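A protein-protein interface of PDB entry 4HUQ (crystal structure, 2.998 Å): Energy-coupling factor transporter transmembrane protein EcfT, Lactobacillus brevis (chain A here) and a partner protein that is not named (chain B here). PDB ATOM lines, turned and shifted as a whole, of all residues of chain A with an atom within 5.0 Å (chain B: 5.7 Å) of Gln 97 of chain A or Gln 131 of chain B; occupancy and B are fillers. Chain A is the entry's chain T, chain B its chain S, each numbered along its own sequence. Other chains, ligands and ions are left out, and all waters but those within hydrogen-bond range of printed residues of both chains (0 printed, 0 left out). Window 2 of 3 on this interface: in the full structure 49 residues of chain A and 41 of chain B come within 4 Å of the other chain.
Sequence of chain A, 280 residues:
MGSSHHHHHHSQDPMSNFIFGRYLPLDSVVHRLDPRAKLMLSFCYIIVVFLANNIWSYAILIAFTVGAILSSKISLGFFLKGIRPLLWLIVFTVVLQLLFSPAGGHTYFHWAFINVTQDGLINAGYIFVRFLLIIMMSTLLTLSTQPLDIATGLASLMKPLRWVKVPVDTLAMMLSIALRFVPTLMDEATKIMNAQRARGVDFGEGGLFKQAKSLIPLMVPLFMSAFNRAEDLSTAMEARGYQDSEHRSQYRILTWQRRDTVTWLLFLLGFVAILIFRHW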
ATOM      1  N   THR A  93      15.344   5.615  -5.213  1.00  0.00           N
ATOM      2  CA  THR A  93      14.954   5.451  -3.819  1.00  0.00           C
ATOM      3  C   THR A  93      14.789   6.803  -3.146  1.00  0.00           C
ATOM      4  O   THR A  93      13.670   7.233  -2.874  1.00  0.00           O
ATOM      5  CB  THR A  93      15.999   4.652  -3.024  1.00  0.00           C
ATOM      6  OG1 THR A  93      17.290   5.253  -3.190  1.00  0.00           O
ATOM      7  CG2 THR A  93      16.056   3.226  -3.507  1.00  0.00           C
ATOM      8  N   VAL A  94      15.915   7.470  -2.898  1.00  0.00           N
ATOM      9  CA  VAL A  94      15.954   8.704  -2.115  1.00  0.00           C
ATOM     10  C   VAL A  94      14.941   9.757  -2.571  1.00  0.00           C
ATOM     11  O   VAL A  94      14.311  10.432  -1.740  1.00  0.00           O
ATOM     12  CB  VAL A  94      17.374   9.304  -2.100  1.00  0.00           C
ATOM     13  CG1 VAL A  94      17.397  10.621  -1.314  1.00  0.00           C
ATOM     14  CG2 VAL A  94      18.358   8.300  -1.511  1.00  0.00           C
ATOM     15  N   VAL A  95      14.774   9.889  -3.885  1.00  0.00           N
ATOM     16  CA  VAL A  95      13.781  10.816  -4.406  1.00  0.00           C
ATOM     17  C   VAL A  95      12.383  10.396  -3.965  1.00  0.00           C
ATOM     18  O   VAL A  95      11.650  11.185  -3.369  1.00  0.00           O
ATOM     19  CB  VAL A  95      13.856  10.945  -5.935  1.00  0.00           C
ATOM     20  CG1 VAL A  95      12.635  11.692  -6.471  1.00  0.00           C
ATOM     21  CG2 VAL A  95      15.133  11.662  -6.319  1.00  0.00           C
ATOM     22  N   LEU A  96      12.043   9.135  -4.224  1.00  0.00           N
ATOM     23  CA  LEU A  96      10.725   8.593  -3.895  1.00  0.00           C
ATOM     24  C   LEU A  96      10.432   8.548  -2.392  1.00  0.00           C
ATOM     25  O   LEU A  96       9.284   8.362  -1.980  1.00  0.00           O
ATOM     26  CB  LEU A  96      10.568   7.195  -4.497  1.00  0.00           C
ATOM     27  CG  LEU A  96       9.812   7.100  -5.821  1.00  0.00           C
ATOM     28  CD1 LEU A  96       8.320   7.158  -5.560  1.00  0.00           C
ATOM     29  CD2 LEU A  96      10.229   8.209  -6.779  1.00  0.00           C
ATOM     30  N   GLN A  97      11.470   8.708  -1.580  1.00  0.00           N
ATOM     31  CA  GLN A  97      11.311   8.706  -0.135  1.00  0.00           C
ATOM     32  C   GLN A  97      11.267  10.132   0.379  1.00  0.00           C
ATOM     33  O   GLN A  97      10.807  10.383   1.492  1.00  0.00           O
ATOM     34  CB  GLN A  97      12.444   7.929   0.543  1.00  0.00           C
ATOM     35  CG  GLN A  97      11.992   6.709   1.354  1.00  0.00           C
ATOM     36  CD  GLN A  97      11.344   7.068   2.691  1.00  0.00           C
ATOM     37  OE1 GLN A  97      10.426   7.891   2.760  1.00  0.00           O
ATOM     38  NE2 GLN A  97      11.824   6.442   3.760  1.00  0.00           N
ATOM     39  N   LEU A  98      11.759  11.062  -0.436  1.00  0.00           N
ATOM     40  CA  LEU A  98      11.659  12.484  -0.126  1.00  0.00           C
ATOM     41  C   LEU A  98      10.226  12.952  -0.342  1.00  0.00           C
ATOM     42  O   LEU A  98       9.568  13.430   0.585  1.00  0.00           O
ATOM     43  CB  LEU A  98      12.623  13.285  -0.991  1.00  0.00           C
ATOM     44  CG  LEU A  98      14.008  13.492  -0.391  1.00  0.00           C
ATOM     45  CD1 LEU A  98      14.890  14.204  -1.399  1.00  0.00           C
ATOM     46  CD2 LEU A  98      13.895  14.284   0.915  1.00  0.00           C
ATOM     47  N   LEU A  99       9.747  12.811  -1.573  1.00  0.00           N
ATOM     48  CA  LEU A  99       8.324  12.919  -1.855  1.00  0.00           C
ATOM     49  C   LEU A  99       7.694  11.662  -1.265  1.00  0.00           C
ATOM     50  O   LEU A  99       8.392  10.673  -1.041  1.00  0.00           O
ATOM     51  CB  LEU A  99       8.076  12.983  -3.367  1.00  0.00           C
ATOM     52  CG  LEU A  99       9.321  13.068  -4.269  1.00  0.00           C
ATOM     53  CD1 LEU A  99       9.142  12.358  -5.623  1.00  0.00           C
ATOM     54  CD2 LEU A  99       9.745  14.515  -4.476  1.00  0.00           C
ATOM     55  N   PHE A 100       6.393  11.704  -0.996  1.00  0.00           N
ATOM     56  CA  PHE A 100       5.671  10.552  -0.443  1.00  0.00           C
ATOM     57  C   PHE A 100       6.123  10.161   0.970  1.00  0.00           C
ATOM     58  O   PHE A 100       6.462   9.001   1.210  1.00  0.00           O
ATOM     59  CB  PHE A 100       5.769   9.328  -1.368  1.00  0.00           C
ATOM     60  CG  PHE A 100       5.448   9.619  -2.805  1.00  0.00           C
ATOM     61  CD1 PHE A 100       4.145   9.882  -3.199  1.00  0.00           C
ATOM     62  CD2 PHE A 100       6.448   9.613  -3.769  1.00  0.00           C
ATOM     63  CE1 PHE A 100       3.845  10.147  -4.526  1.00  0.00           C
ATOM     64  CE2 PHE A 100       6.157   9.875  -5.102  1.00  0.00           C
ATOM     65  CZ  PHE A 100       4.855  10.140  -5.480  1.00  0.00           C
ATOM     66  N   SER A 101       6.112  11.116   1.903  1.00  0.00           N
ATOM     67  CA  SER A 101       6.493  10.833   3.290  1.00  0.00           C
ATOM     68  C   SER A 101       5.859  11.769   4.317  1.00  0.00           C
ATOM     69  O   SER A 101       5.788  11.448   5.508  1.00  0.00           O
ATOM     70  CB  SER A 101       8.016  10.838   3.438  1.00  0.00           C
ATOM     71  OG  SER A 101       8.592   9.752   2.725  1.00  0.00           O
ATOM     72  N   GLY A 120      11.621  13.250   6.689  1.00  0.00           N
ATOM     73  CA  GLY A 120      11.902  12.505   5.476  1.00  0.00           C
ATOM     74  C   GLY A 120      13.299  12.744   4.935  1.00  0.00           C
ATOM     75  O   GLY A 120      13.967  11.806   4.503  1.00  0.00           O
ATOM     76  N   ASN A 123      15.459  10.597   6.749  1.00  0.00           N
ATOM     77  CA  ASN A 123      15.498   9.231   6.228  1.00  0.00           C
ATOM     78  C   ASN A 123      16.551   8.994   5.146  1.00  0.00           C
ATOM     79  O   ASN A 123      17.227   7.966   5.145  1.00  0.00           O
ATOM     80  CB  ASN A 123      14.121   8.832   5.696  1.00  0.00           C
ATOM     81  CG  ASN A 123      13.574   7.592   6.370  1.00  0.00           C
ATOM     82  OD1 ASN A 123      12.676   6.934   5.847  1.00  0.00           O
ATOM     83  ND2 ASN A 123      14.114   7.266   7.537  1.00  0.00           N
ATOM     84  N   ILE A 127      19.144   5.901   4.362  1.00  0.00           N
ATOM     85  CA  ILE A 127      19.208   5.166   3.109  1.00  0.00           C
ATOM     86  C   ILE A 127      20.399   5.521   2.229  1.00  0.00           C
ATOM     87  O   ILE A 127      21.073   4.626   1.708  1.00  0.00           O
ATOM     88  CB  ILE A 127      17.908   5.373   2.329  1.00  0.00           C
ATOM     89  CG1 ILE A 127      16.745   4.780   3.109  1.00  0.00           C
ATOM     90  CG2 ILE A 127      17.965   4.717   0.986  1.00  0.00           C
ATOM     91  CD1 ILE A 127      15.425   5.411   2.773  1.00  0.00           C
ATOM     92  N   ARG A 130      23.135   4.260   4.143  1.00  0.00           N
ATOM     93  CA  ARG A 130      22.952   2.813   4.139  1.00  0.00           C
ATOM     94  C   ARG A 130      23.370   2.206   2.809  1.00  0.00           C
ATOM     95  O   ARG A 130      24.016   1.166   2.770  1.00  0.00           O
ATOM     96  CB  ARG A 130      21.492   2.458   4.414  1.00  0.00           C
ATOM     97  CG  ARG A 130      21.288   1.026   4.858  1.00  0.00           C
ATOM     98  CD  ARG A 130      20.433   0.217   3.895  1.00  0.00           C
ATOM     99  NE  ARG A 130      19.781  -0.875   4.613  1.00  0.00           N
ATOM    100  CZ  ARG A 130      18.466  -0.995   4.772  1.00  0.00           C
ATOM    101  NH1 ARG A 130      17.640  -0.108   4.232  1.00  0.00           N
ATOM    102  NH2 ARG A 130      17.974  -2.021   5.456  1.00  0.00           N
ATOM    103  N   TRP B 125      15.631  -6.939  -2.792  1.00  0.00           N
ATOM    104  CA  TRP B 125      16.272  -5.648  -2.545  1.00  0.00           C
ATOM    105  C   TRP B 125      15.373  -4.724  -1.759  1.00  0.00           C
ATOM    106  O   TRP B 125      15.857  -3.913  -0.977  1.00  0.00           O
ATOM    107  CB  TRP B 125      16.760  -4.964  -3.823  1.00  0.00           C
ATOM    108  CG  TRP B 125      15.780  -4.955  -4.919  1.00  0.00           C
ATOM    109  CD1 TRP B 125      14.651  -4.202  -5.002  1.00  0.00           C
ATOM    110  CD2 TRP B 125      15.844  -5.726  -6.121  1.00  0.00           C
ATOM    111  NE1 TRP B 125      13.997  -4.465  -6.183  1.00  0.00           N
ATOM    112  CE2 TRP B 125      14.712  -5.396  -6.890  1.00  0.00           C
ATOM    113  CE3 TRP B 125      16.751  -6.668  -6.624  1.00  0.00           C
ATOM    114  CZ2 TRP B 125      14.458  -5.975  -8.135  1.00  0.00           C
ATOM    115  CZ3 TRP B 125      16.498  -7.242  -7.862  1.00  0.00           C
ATOM    116  CH2 TRP B 125      15.360  -6.896  -8.600  1.00  0.00           C
ATOM    117  N   VAL B 126      14.069  -4.850  -1.969  1.00  0.00           N
ATOM    118  CA  VAL B 126      13.114  -4.150  -1.127  1.00  0.00           C
ATOM    119  C   VAL B 126      13.388  -4.531   0.318  1.00  0.00           C
ATOM    120  O   VAL B 126      13.312  -3.683   1.211  1.00  0.00           O
ATOM    121  CB  VAL B 126      11.660  -4.485  -1.489  1.00  0.00           C
ATOM    122  CG1 VAL B 126      10.697  -3.730  -0.579  1.00  0.00           C
ATOM    123  CG2 VAL B 126      11.397  -4.141  -2.943  1.00  0.00           C
ATOM    124  N   ILE B 128      15.461  -4.975   3.429  1.00  0.00           N
ATOM    125  CA  ILE B 128      16.665  -4.717   4.227  1.00  0.00           C
ATOM    126  C   ILE B 128      18.017  -4.466   3.522  1.00  0.00           C
ATOM    127  O   ILE B 128      18.901  -3.838   4.104  1.00  0.00           O
ATOM    128  CB  ILE B 128      16.826  -5.826   5.293  1.00  0.00           C
ATOM    129  CG1 ILE B 128      17.143  -7.170   4.627  1.00  0.00           C
ATOM    130  CG2 ILE B 128      15.568  -5.922   6.156  1.00  0.00           C
ATOM    131  CD1 ILE B 128      16.924  -8.372   5.520  1.00  0.00           C
ATOM    132  N   MET B 129      18.188  -4.973   2.303  1.00  0.00           N
ATOM    133  CA  MET B 129      19.340  -4.636   1.476  1.00  0.00           C
ATOM    134  C   MET B 129      19.289  -3.155   1.219  1.00  0.00           C
ATOM    135  O   MET B 129      20.174  -2.405   1.626  1.00  0.00           O
ATOM    136  CB  MET B 129      19.270  -5.367   0.146  1.00  0.00           C
ATOM    137  CG  MET B 129      19.814  -6.769   0.193  1.00  0.00           C
ATOM    138  SD  MET B 129      20.903  -7.080  -1.225  1.00  0.00           S
ATOM    139  CE  MET B 129      22.087  -5.750  -1.014  1.00  0.00           C
ATOM    140  N   TYR B 130      18.232  -2.741   0.532  1.00  0.00           N
ATOM    141  CA  TYR B 130      17.931  -1.330   0.368  1.00  0.00           C
ATOM    142  C   TYR B 130      16.484  -1.129   0.801  1.00  0.00           C
ATOM    143  O   TYR B 130      15.729  -2.091   0.895  1.00  0.00           O
ATOM    144  CB  TYR B 130      18.146  -0.921  -1.082  1.00  0.00           C
ATOM    145  CG  TYR B 130      19.339  -1.618  -1.717  1.00  0.00           C
ATOM    146  CD1 TYR B 130      20.621  -1.472  -1.192  1.00  0.00           C
ATOM    147  CD2 TYR B 130      19.184  -2.412  -2.842  1.00  0.00           C
ATOM    148  CE1 TYR B 130      21.710  -2.111  -1.760  1.00  0.00           C
ATOM    149  CE2 TYR B 130      20.267  -3.049  -3.421  1.00  0.00           C
ATOM    150  CZ  TYR B 130      21.529  -2.895  -2.875  1.00  0.00           C
ATOM    151  OH  TYR B 130      22.611  -3.531  -3.453  1.00  0.00           O
ATOM    152  N   GLN B 131      16.090   0.101   1.096  1.00  0.00           N
ATOM    153  CA  GLN B 131      14.733   0.314   1.574  1.00  0.00           C
ATOM    154  C   GLN B 131      13.736   0.240   0.432  1.00  0.00           C
ATOM    155  O   GLN B 131      12.575  -0.087   0.658  1.00  0.00           O
ATOM    156  CB  GLN B 131      14.591   1.668   2.270  1.00  0.00           C
ATOM    157  CG  GLN B 131      13.878   2.732   1.420  1.00  0.00           C
ATOM    158  CD  GLN B 131      12.398   2.898   1.752  1.00  0.00           C
ATOM    159  OE1 GLN B 131      12.037   3.618   2.686  1.00  0.00           O
ATOM    160  NE2 GLN B 131      11.537   2.247   0.973  1.00  0.00           N
ATOM    161  N   THR B 132      14.208   0.552  -0.776  1.00  0.00           N
ATOM    162  CA  THR B 132      13.371   0.783  -1.961  1.00  0.00           C
ATOM    163  C   THR B 132      11.948   0.188  -1.949  1.00  0.00           C
ATOM    164  O   THR B 132      11.774  -1.024  -1.803  1.00  0.00           O
ATOM    165  CB  THR B 132      14.112   0.369  -3.250  1.00  0.00           C
ATOM    166  OG1 THR B 132      13.187   0.293  -4.341  1.00  0.00           O
ATOM    167  CG2 THR B 132      14.805  -0.969  -3.067  1.00  0.00           C
ATOM    168  N   PRO B 133      10.931   1.057  -2.102  1.00  0.00           N
ATOM    169  CA  PRO B 133       9.495   0.750  -2.008  1.00  0.00           C
ATOM    170  C   PRO B 133       9.048  -0.345  -2.974  1.00  0.00           C
ATOM    171  O   PRO B 133       9.246  -0.224  -4.185  1.00  0.00           O
ATOM    172  CB  PRO B 133       8.831   2.079  -2.382  1.00  0.00           C
ATOM    173  CG  PRO B 133       9.871   2.819  -3.169  1.00  0.00           C
ATOM    174  CD  PRO B 133      11.162   2.452  -2.516  1.00  0.00           C
ATOM    175  N   PHE B 134       8.429  -1.392  -2.435  1.00  0.00           N
ATOM    176  CA  PHE B 134       8.088  -2.569  -3.224  1.00  0.00           C
ATOM    177  C   PHE B 134       7.108  -2.273  -4.351  1.00  0.00           C
ATOM    178  O   PHE B 134       7.465  -2.374  -5.530  1.00  0.00           O
ATOM    179  CB  PHE B 134       7.531  -3.682  -2.338  1.00  0.00           C
ATOM    180  CG  PHE B 134       7.302  -4.971  -3.069  1.00  0.00           C
ATOM    181  CD1 PHE B 134       8.342  -5.862  -3.264  1.00  0.00           C
ATOM    182  CD2 PHE B 134       6.051  -5.291  -3.572  1.00  0.00           C
ATOM    183  CE1 PHE B 134       8.142  -7.050  -3.944  1.00  0.00           C
ATOM    184  CE2 PHE B 134       5.843  -6.477  -4.251  1.00  0.00           C
ATOM    185  CZ  PHE B 134       6.890  -7.358  -4.437  1.00  0.00           C
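Hydrophobic or aromatic side chains of chain A that line the printed part of chain B: Ile 127. Hydrophobic or aromatic side chains of chain B that line the printed part of chain A: Ile 128. Along chain B the printed residues that touch a printed residue of chain A span positions 128 to 132. Among the printed residues, 7 pairs touch across the chains. Among the printed residues, no Asp or Glu carboxylate lies within 4 Å of a Lys or Arg side-chain nitrogen of the other chain.
Thr 93 of chain A touches Thr 132 of chain B. CG of Gln 131 of chain B touches CD1 of Ile 127 of chain A, at 3.4 Å. Arg 130 of chain A touches Tyr 130 of chain B. Arg 130 of chain A touches Gln 131 of chain B (NH1 to N, 3.5 Å).
O of Met 129 of chain B is in hydrogen-bond range of NE of Arg 130 of chain A (3.4 Å). NE2 of Gln 97 of chain A sits at hydrogen-bond distance from OE1 of Gln 131 of chain B (3.0 Å). O of Ile 128 of chain B lies within hydrogen-bond range of NH2 of Arg 130 of chain A, 2.4 Å away.
The backbone carbonyl oxygen (O) of Gln 97 of chain A sits at hydrogen-bond distance from the side-chain hydroxyl (OG) of Ser 101 of chain A (2.6 Å). The backbone carbonyl oxygen (O) of Trp 125 of chain B sits at hydrogen-bond distance from the backbone NH (N) of Tyr 130 of chain B, 3.0 Å away.
Of chain B, only Gln 131 comes within 4 Å of Gln 97 of chain A. Trp 125 of chain B touches none of the printed residues of chain A. Of the printed residues of chain A, Ile 128 of chain B touches Arg 130 (2.4 Å). Printed residues of chain A within 4 Å of Met 129 of chain B: Arg 130. Of the printed residues of chain A, Gln 131 of chain B touches Gln 97 (3.0 Å), Ile 127 (3.4 Å) and Arg 130 (3.5 Å). The nearest residue of chain A that does not touch Gln 131 of chain B is Asn 123 of chain A (4.6 Å).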
